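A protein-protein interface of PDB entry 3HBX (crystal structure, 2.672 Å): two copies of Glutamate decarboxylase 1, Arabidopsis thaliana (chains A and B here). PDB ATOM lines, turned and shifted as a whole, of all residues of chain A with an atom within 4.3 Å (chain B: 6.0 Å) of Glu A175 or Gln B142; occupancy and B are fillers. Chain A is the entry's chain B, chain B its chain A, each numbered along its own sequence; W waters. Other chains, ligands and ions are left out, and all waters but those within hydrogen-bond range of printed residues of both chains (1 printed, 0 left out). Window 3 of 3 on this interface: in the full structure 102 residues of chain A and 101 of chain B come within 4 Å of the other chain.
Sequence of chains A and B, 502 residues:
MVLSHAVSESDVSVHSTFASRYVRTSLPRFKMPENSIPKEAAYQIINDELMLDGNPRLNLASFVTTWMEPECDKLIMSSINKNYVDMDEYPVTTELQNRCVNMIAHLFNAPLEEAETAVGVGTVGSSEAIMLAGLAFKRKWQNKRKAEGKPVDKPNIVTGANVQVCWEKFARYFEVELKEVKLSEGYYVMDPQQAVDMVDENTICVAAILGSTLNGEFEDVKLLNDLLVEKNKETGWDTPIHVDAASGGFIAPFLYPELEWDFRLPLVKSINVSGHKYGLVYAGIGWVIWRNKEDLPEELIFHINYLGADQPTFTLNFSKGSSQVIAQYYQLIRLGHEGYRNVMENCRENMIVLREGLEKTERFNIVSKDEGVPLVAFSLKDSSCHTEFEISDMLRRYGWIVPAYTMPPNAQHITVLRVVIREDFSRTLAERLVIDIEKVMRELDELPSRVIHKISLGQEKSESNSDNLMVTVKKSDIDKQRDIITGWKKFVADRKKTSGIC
NE2 of Gln B142 lies within hydrogen-bond range of OE2 of Glu A175.
The side-chain amino group (NZ) of Lys B138 is in salt-bridge range of the side-chain carboxylate (OE2) of Glu A175 (3.0 Å).
NZ of Lys B138 lies within hydrogen-bond range of O of Phe B174 (2.9 Å).
Among the printed residues, merely in contact across the chains: Phe A174 with Phe B174, Tyr A173 with Phe B174 and Arg A172 with Arg B139.
Of the printed residues of chain B, Arg A172 touches Arg B139 (3.7 Å).
Printed residues of chain B within 4 Å of Tyr A173: Phe B174 (3.6 Å).
Printed residues of chain B within 4 Å of Phe A174: Phe B174 (3.3 Å).
Of chain B, only Lys B138 (3.0 Å) and Gln B142 (2.9 Å) come within 4 Å of Glu A175.
Of chain A, only Glu A175 (2.9 Å) comes within 4 Å of Gln B142.
The nearest printed residue of chain A that does not touch Gln B142 is Arg A172 (7.1 Å).
Of the 8 printed residues of chain A, 4 touch a printed residue of chain B.
Of the 15 printed residues of chain B, 4 touch a printed residue of chain A.
Printed residues of chain B that touch a printed residue of chain A: Lys B138, Arg B139, Gln B142 and Phe B174.
Among the printed residues, 5 pairs touch across the chains.
Among the printed residues, Asp or Glu carboxylates within 4 Å of a Lys or Arg side-chain nitrogen of the other chain: Glu A175 with Lys B138.
Phe A174 touches its own counterpart, Phe B174.
Of the 5 pairs that touch across the chains among the printed residues, 1 has its exchanged pair printed and touching as well.
Water W1 lies within hydrogen-bond range of the guanidinium group of Arg B139 (2.7 Å) and the side-chain carboxylate of Glu A175 (3.4 Å).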
ATOM      1  N   PRO A 155      15.716   9.589  -0.276  1.00  0.00           N
ATOM      2  CA  PRO A 155      14.714  10.084  -1.226  1.00  0.00           C
ATOM      3  C   PRO A 155      13.350  10.209  -0.559  1.00  0.00           C
ATOM      4  O   PRO A 155      13.067   9.487   0.398  1.00  0.00           O
ATOM      5  CB  PRO A 155      14.666   8.984  -2.295  1.00  0.00           C
ATOM      6  CG  PRO A 155      15.823   8.065  -2.000  1.00  0.00           C
ATOM      7  CD  PRO A 155      16.082   8.192  -0.542  1.00  0.00           C
ATOM      8  N   PHE A 170       4.849   1.477  -2.353  1.00  0.00           N
ATOM      9  CA  PHE A 170       6.042   1.921  -3.063  1.00  0.00           C
ATOM     10  C   PHE A 170       7.086   2.461  -2.097  1.00  0.00           C
ATOM     11  O   PHE A 170       8.246   2.053  -2.132  1.00  0.00           O
ATOM     12  CB  PHE A 170       5.700   2.986  -4.104  1.00  0.00           C
ATOM     13  CG  PHE A 170       6.904   3.659  -4.692  1.00  0.00           C
ATOM     14  CD1 PHE A 170       7.660   3.025  -5.664  1.00  0.00           C
ATOM     15  CD2 PHE A 170       7.292   4.918  -4.263  1.00  0.00           C
ATOM     16  CE1 PHE A 170       8.779   3.635  -6.204  1.00  0.00           C
ATOM     17  CE2 PHE A 170       8.409   5.537  -4.797  1.00  0.00           C
ATOM     18  CZ  PHE A 170       9.155   4.894  -5.770  1.00  0.00           C
ATOM     19  N   ALA A 171       6.664   3.380  -1.234  1.00  0.00           N
ATOM     20  CA  ALA A 171       7.567   3.999  -0.271  1.00  0.00           C
ATOM     21  C   ALA A 171       8.294   2.955   0.567  1.00  0.00           C
ATOM     22  O   ALA A 171       9.510   3.016   0.729  1.00  0.00           O
ATOM     23  CB  ALA A 171       6.806   4.965   0.627  1.00  0.00           C
ATOM     24  N   ARG A 172       7.544   1.991   1.088  1.00  0.00           N
ATOM     25  CA  ARG A 172       8.109   0.980   1.972  1.00  0.00           C
ATOM     26  C   ARG A 172       9.008  -0.018   1.242  1.00  0.00           C
ATOM     27  O   ARG A 172      10.092  -0.346   1.720  1.00  0.00           O
ATOM     28  CB  ARG A 172       6.995   0.238   2.710  1.00  0.00           C
ATOM     29  CG  ARG A 172       7.493  -0.773   3.725  1.00  0.00           C
ATOM     30  CD  ARG A 172       6.343  -1.306   4.560  1.00  0.00           C
ATOM     31  NE  ARG A 172       5.639  -0.238   5.263  1.00  0.00           N
ATOM     32  CZ  ARG A 172       4.490  -0.399   5.912  1.00  0.00           C
ATOM     33  NH1 ARG A 172       3.905  -1.589   5.947  1.00  0.00           N
ATOM     34  NH2 ARG A 172       3.922   0.633   6.523  1.00  0.00           N
ATOM     35  N   TYR A 173       8.556  -0.503   0.091  1.00  0.00           N
ATOM     36  CA  TYR A 173       9.298  -1.534  -0.630  1.00  0.00           C
ATOM     37  C   TYR A 173      10.520  -0.983  -1.361  1.00  0.00           C
ATOM     38  O   TYR A 173      11.536  -1.667  -1.491  1.00  0.00           O
ATOM     39  CB  TYR A 173       8.391  -2.284  -1.611  1.00  0.00           C
ATOM     40  CG  TYR A 173       7.197  -2.940  -0.957  1.00  0.00           C
ATOM     41  CD1 TYR A 173       7.222  -3.281   0.387  1.00  0.00           C
ATOM     42  CD2 TYR A 173       6.054  -3.235  -1.687  1.00  0.00           C
ATOM     43  CE1 TYR A 173       6.137  -3.883   0.991  1.00  0.00           C
ATOM     44  CE2 TYR A 173       4.965  -3.838  -1.091  1.00  0.00           C
ATOM     45  CZ  TYR A 173       5.014  -4.159   0.247  1.00  0.00           C
ATOM     46  OH  TYR A 173       3.934  -4.761   0.850  1.00  0.00           O
ATOM     47  N   PHE A 174      10.421   0.253  -1.838  1.00  0.00           N
ATOM     48  CA  PHE A 174      11.524   0.867  -2.566  1.00  0.00           C
ATOM     49  C   PHE A 174      12.271   1.884  -1.711  1.00  0.00           C
ATOM     50  O   PHE A 174      13.017   2.718  -2.224  1.00  0.00           O
ATOM     51  CB  PHE A 174      11.025   1.487  -3.873  1.00  0.00           C
ATOM     52  CG  PHE A 174      10.478   0.477  -4.839  1.00  0.00           C
ATOM     53  CD1 PHE A 174      11.322  -0.202  -5.703  1.00  0.00           C
ATOM     54  CD2 PHE A 174       9.123   0.189  -4.869  1.00  0.00           C
ATOM     55  CE1 PHE A 174      10.823  -1.141  -6.586  1.00  0.00           C
ATOM     56  CE2 PHE A 174       8.619  -0.749  -5.752  1.00  0.00           C
ATOM     57  CZ  PHE A 174       9.471  -1.414  -6.612  1.00  0.00           C
ATOM     58  N   GLU A 175      12.064   1.796  -0.401  1.00  0.00           N
ATOM     59  CA  GLU A 175      12.803   2.600   0.565  1.00  0.00           C
ATOM     60  C   GLU A 175      12.830   4.085   0.209  1.00  0.00           C
ATOM     61  O   GLU A 175      13.893   4.686   0.067  1.00  0.00           O
ATOM     62  CB  GLU A 175      14.221   2.049   0.740  1.00  0.00           C
ATOM     63  CG  GLU A 175      14.243   0.664   1.371  1.00  0.00           C
ATOM     64  CD  GLU A 175      15.556  -0.065   1.168  1.00  0.00           C
ATOM     65  OE1 GLU A 175      16.563   0.592   0.828  1.00  0.00           O
ATOM     66  OE2 GLU A 175      15.578  -1.302   1.350  1.00  0.00           O
ATOM     67  N   VAL A 176      11.643   4.660   0.062  1.00  0.00           N
ATOM     68  CA  VAL A 176      11.497   6.088  -0.164  1.00  0.00           C
ATOM     69  C   VAL A 176      10.602   6.648   0.932  1.00  0.00           C
ATOM     70  O   VAL A 176       9.649   5.996   1.353  1.00  0.00           O
ATOM     71  CB  VAL A 176      10.875   6.383  -1.542  1.00  0.00           C
ATOM     72  CG1 VAL A 176      10.629   7.875  -1.707  1.00  0.00           C
ATOM     73  CG2 VAL A 176      11.772   5.857  -2.656  1.00  0.00           C
ATOM     74  N   PHE B 137      13.411 -11.502   1.852  1.00  0.00           N
ATOM     75  CA  PHE B 137      14.806 -11.831   2.114  1.00  0.00           C
ATOM     76  C   PHE B 137      15.614 -10.586   2.465  1.00  0.00           C
ATOM     77  O   PHE B 137      16.334 -10.567   3.460  1.00  0.00           O
ATOM     78  CB  PHE B 137      15.440 -12.544   0.915  1.00  0.00           C
ATOM     79  CG  PHE B 137      15.097 -13.999   0.828  1.00  0.00           C
ATOM     80  CD1 PHE B 137      15.301 -14.834   1.913  1.00  0.00           C
ATOM     81  CD2 PHE B 137      14.578 -14.537  -0.339  1.00  0.00           C
ATOM     82  CE1 PHE B 137      14.985 -16.179   1.841  1.00  0.00           C
ATOM     83  CE2 PHE B 137      14.264 -15.880  -0.418  1.00  0.00           C
ATOM     84  CZ  PHE B 137      14.467 -16.702   0.674  1.00  0.00           C
ATOM     85  N   LYS B 138      15.490  -9.554   1.638  1.00  0.00           N
ATOM     86  CA  LYS B 138      16.238  -8.321   1.839  1.00  0.00           C
ATOM     87  C   LYS B 138      15.925  -7.722   3.200  1.00  0.00           C
ATOM     88  O   LYS B 138      16.827  -7.409   3.972  1.00  0.00           O
ATOM     89  CB  LYS B 138      15.916  -7.310   0.737  1.00  0.00           C
ATOM     90  CG  LYS B 138      16.765  -6.052   0.790  1.00  0.00           C
ATOM     91  CD  LYS B 138      16.325  -5.035  -0.250  1.00  0.00           C
ATOM     92  CE  LYS B 138      17.226  -3.811  -0.222  1.00  0.00           C
ATOM     93  NZ  LYS B 138      16.709  -2.709  -1.076  1.00  0.00           N
ATOM     94  N   ARG B 139      14.637  -7.572   3.490  1.00  0.00           N
ATOM     95  CA  ARG B 139      14.191  -6.982   4.743  1.00  0.00           C
ATOM     96  C   ARG B 139      14.646  -7.813   5.939  1.00  0.00           C
ATOM     97  O   ARG B 139      15.180  -7.279   6.910  1.00  0.00           O
ATOM     98  CB  ARG B 139      12.668  -6.836   4.748  1.00  0.00           C
ATOM     99  CG  ARG B 139      12.134  -5.873   5.796  1.00  0.00           C
ATOM    100  CD  ARG B 139      12.888  -4.552   5.756  1.00  0.00           C
ATOM    101  NE  ARG B 139      12.054  -3.429   6.172  1.00  0.00           N
ATOM    102  CZ  ARG B 139      11.521  -2.545   5.332  1.00  0.00           C
ATOM    103  NH1 ARG B 139      11.741  -2.649   4.026  1.00  0.00           N
ATOM    104  NH2 ARG B 139      10.772  -1.555   5.799  1.00  0.00           N
ATOM    105  N   LYS B 140      14.433  -9.122   5.863  1.00  0.00           N
ATOM    106  CA  LYS B 140      14.828 -10.021   6.940  1.00  0.00           C
ATOM    107  C   LYS B 140      16.329  -9.916   7.194  1.00  0.00           C
ATOM    108  O   LYS B 140      16.791 -10.016   8.330  1.00  0.00           O
ATOM    109  CB  LYS B 140      14.449 -11.461   6.593  1.00  0.00           C
ATOM    110  CG  LYS B 140      14.449 -12.409   7.776  1.00  0.00           C
ATOM    111  CD  LYS B 140      13.957 -13.788   7.372  1.00  0.00           C
ATOM    112  CE  LYS B 140      13.685 -14.662   8.585  1.00  0.00           C
ATOM    113  NZ  LYS B 140      14.916 -14.951   9.365  1.00  0.00           N
ATOM    114  N   TRP B 141      17.082  -9.706   6.119  1.00  0.00           N
ATOM    115  CA  TRP B 141      18.530  -9.568   6.193  1.00  0.00           C
ATOM    116  C   TRP B 141      18.913  -8.215   6.789  1.00  0.00           C
ATOM    117  O   TRP B 141      19.793  -8.130   7.647  1.00  0.00           O
ATOM    118  CB  TRP B 141      19.135  -9.739   4.797  1.00  0.00           C
ATOM    119  CG  TRP B 141      20.601  -9.446   4.696  1.00  0.00           C
ATOM    120  CD1 TRP B 141      21.630 -10.295   4.987  1.00  0.00           C
ATOM    121  CD2 TRP B 141      21.204  -8.224   4.250  1.00  0.00           C
ATOM    122  NE1 TRP B 141      22.834  -9.674   4.759  1.00  0.00           N
ATOM    123  CE2 TRP B 141      22.600  -8.402   4.306  1.00  0.00           C
ATOM    124  CE3 TRP B 141      20.698  -6.994   3.816  1.00  0.00           C
ATOM    125  CZ2 TRP B 141      23.495  -7.398   3.947  1.00  0.00           C
ATOM    126  CZ3 TRP B 141      21.588  -6.001   3.458  1.00  0.00           C
ATOM    127  CH2 TRP B 141      22.970  -6.208   3.526  1.00  0.00           C
ATOM    128  N   GLN B 142      18.243  -7.160   6.337  1.00  0.00           N
ATOM    129  CA  GLN B 142      18.469  -5.824   6.870  1.00  0.00           C
ATOM    130  C   GLN B 142      18.243  -5.796   8.377  1.00  0.00           C
ATOM    131  O   GLN B 142      19.071  -5.284   9.124  1.00  0.00           O
ATOM    132  CB  GLN B 142      17.550  -4.809   6.186  1.00  0.00           C
ATOM    133  CG  GLN B 142      17.929  -4.491   4.749  1.00  0.00           C
ATOM    134  CD  GLN B 142      16.913  -3.595   4.065  1.00  0.00           C
ATOM    135  OE1 GLN B 142      15.761  -3.510   4.488  1.00  0.00           O
ATOM    136  NE2 GLN B 142      17.336  -2.926   3.000  1.00  0.00           N
ATOM    137  N   ASN B 143      17.116  -6.349   8.816  1.00  0.00           N
ATOM    138  CA  ASN B 143      16.791  -6.396  10.240  1.00  0.00           C
ATOM    139  C   ASN B 143      17.872  -7.104  11.049  1.00  0.00           C
ATOM    140  O   ASN B 143      18.321  -6.602  12.078  1.00  0.00           O
ATOM    141  CB  ASN B 143      15.441  -7.083  10.467  1.00  0.00           C
ATOM    142  CG  ASN B 143      14.267  -6.215  10.059  1.00  0.00           C
ATOM    143  OD1 ASN B 143      14.407  -5.004   9.879  1.00  0.00           O
ATOM    144  ND2 ASN B 143      13.100  -6.832   9.913  1.00  0.00           N
ATOM    145  N   LYS B 144      18.284  -8.273  10.570  1.00  0.00           N
ATOM    146  CA  LYS B 144      19.281  -9.080  11.260  1.00  0.00           C
ATOM    147  C   LYS B 144      20.593  -8.322  11.401  1.00  0.00           C
ATOM    148  O   LYS B 144      21.233  -8.364  12.448  1.00  0.00           O
ATOM    149  CB  LYS B 144      19.515 -10.390  10.507  1.00  0.00           C
ATOM    150  CG  LYS B 144      20.371 -11.394  11.257  1.00  0.00           C
ATOM    151  CD  LYS B 144      20.659 -12.624  10.405  1.00  0.00           C
ATOM    152  CE  LYS B 144      21.483 -12.270   9.174  1.00  0.00           C
ATOM    153  NZ  LYS B 144      21.867 -13.479   8.389  1.00  0.00           N
ATOM    154  N   ARG B 145      20.983  -7.626  10.340  1.00  0.00           N
ATOM    155  CA  ARG B 145      22.235  -6.877  10.331  1.00  0.00           C
ATOM    156  C   ARG B 145      22.160  -5.627  11.208  1.00  0.00           C
ATOM    157  O   ARG B 145      23.075  -5.354  11.983  1.00  0.00           O
ATOM    158  CB  ARG B 145      22.615  -6.496   8.900  1.00  0.00           C
ATOM    159  CG  ARG B 145      22.858  -7.686   7.983  1.00  0.00           C
ATOM    160  CD  ARG B 145      24.309  -8.135   8.010  1.00  0.00           C
ATOM    161  NE  ARG B 145      25.184  -7.158   7.363  1.00  0.00           N
ATOM    162  CZ  ARG B 145      26.489  -7.329   7.166  1.00  0.00           C
ATOM    163  NH1 ARG B 145      27.083  -8.446   7.566  1.00  0.00           N
ATOM    164  NH2 ARG B 145      27.200  -6.383   6.568  1.00  0.00           N
ATOM    165  N   LYS B 146      21.076  -4.868  11.079  1.00  0.00           N
ATOM    166  CA  LYS B 146      20.887  -3.676  11.895  1.00  0.00           C
ATOM    167  C   LYS B 146      20.925  -4.027  13.379  1.00  0.00           C
ATOM    168  O   LYS B 146      21.357  -3.222  14.204  1.00  0.00           O
ATOM    169  CB  LYS B 146      19.566  -2.986  11.552  1.00  0.00           C
ATOM    170  CG  LYS B 146      19.571  -2.230  10.233  1.00  0.00           C
ATOM    171  CD  LYS B 146      18.173  -1.718   9.891  1.00  0.00           C
ATOM    172  CE  LYS B 146      18.139  -1.058   8.518  1.00  0.00           C
ATOM    173  NZ  LYS B 146      16.747  -0.827   8.032  1.00  0.00           N
ATOM    174  N   ALA B 147      20.473  -5.232  13.712  1.00  0.00           N
ATOM    175  CA  ALA B 147      20.457  -5.691  15.097  1.00  0.00           C
ATOM    176  C   ALA B 147      21.868  -6.008  15.579  1.00  0.00           C
ATOM    177  O   ALA B 147      22.147  -5.986  16.778  1.00  0.00           O
ATOM    178  CB  ALA B 147      19.556  -6.909  15.244  1.00  0.00           C
ATOM    179  N   VAL B 152      24.321  -2.389   5.903  1.00  0.00           N
ATOM    180  CA  VAL B 152      23.292  -3.009   5.078  1.00  0.00           C
ATOM    181  C   VAL B 152      23.173  -2.338   3.715  1.00  0.00           C
ATOM    182  O   VAL B 152      22.087  -2.275   3.141  1.00  0.00           O
ATOM    183  CB  VAL B 152      21.921  -2.949   5.773  1.00  0.00           C
ATOM    184  CG1 VAL B 152      21.958  -3.707   7.090  1.00  0.00           C
ATOM    185  CG2 VAL B 152      21.507  -1.504   5.999  1.00  0.00           C
ATOM    186  N   PRO B 155      23.596  -5.436  -0.368  1.00  0.00           N
ATOM    187  CA  PRO B 155      22.982  -6.768  -0.389  1.00  0.00           C
ATOM    188  C   PRO B 155      23.237  -7.463  -1.721  1.00  0.00           C
ATOM    189  O   PRO B 155      23.398  -6.791  -2.738  1.00  0.00           O
ATOM    190  CB  PRO B 155      21.483  -6.470  -0.251  1.00  0.00           C
ATOM    191  CG  PRO B 155      21.376  -5.009   0.079  1.00  0.00           C
ATOM    192  CD  PRO B 155      22.592  -4.369  -0.489  1.00  0.00           C
ATOM    193  N   PHE B 174      15.285  -3.170  -6.970  1.00  0.00           N
ATOM    194  CA  PHE B 174      15.392  -3.154  -5.515  1.00  0.00           C
ATOM    195  C   PHE B 174      16.840  -3.029  -5.051  1.00  0.00           C
ATOM    196  O   PHE B 174      17.163  -3.312  -3.896  1.00  0.00           O
ATOM    197  CB  PHE B 174      14.714  -4.385  -4.914  1.00  0.00           C
ATOM    198  CG  PHE B 174      13.236  -4.431  -5.163  1.00  0.00           C
ATOM    199  CD1 PHE B 174      12.358  -3.765  -4.321  1.00  0.00           C
ATOM    200  CD2 PHE B 174      12.722  -5.113  -6.251  1.00  0.00           C
ATOM    201  CE1 PHE B 174      10.998  -3.793  -4.553  1.00  0.00           C
ATOM    202  CE2 PHE B 174      11.362  -5.144  -6.485  1.00  0.00           C
ATOM    203  CZ  PHE B 174      10.499  -4.484  -5.636  1.00  0.00           C
ATOM    204  N   GLU B 175      17.703  -2.603  -5.969  1.00  0.00           N
ATOM    205  CA  GLU B 175      19.094  -2.299  -5.659  1.00  0.00           C
ATOM    206  C   GLU B 175      19.782  -3.409  -4.873  1.00  0.00           C
ATOM    207  O   GLU B 175      20.304  -3.187  -3.783  1.00  0.00           O
ATOM    208  CB  GLU B 175      19.185  -0.960  -4.923  1.00  0.00           C
ATOM    209  CG  GLU B 175      18.772   0.220  -5.793  1.00  0.00           C
ATOM    210  CD  GLU B 175      18.470   1.473  -4.995  1.00  0.00           C
ATOM    211  OE1 GLU B 175      18.868   1.545  -3.812  1.00  0.00           O
ATOM    212  OE2 GLU B 175      17.830   2.386  -5.557  1.00  0.00           O
HETATM  213  O   HOH W   1      13.148  -3.562   1.958  1.00  0.00           O
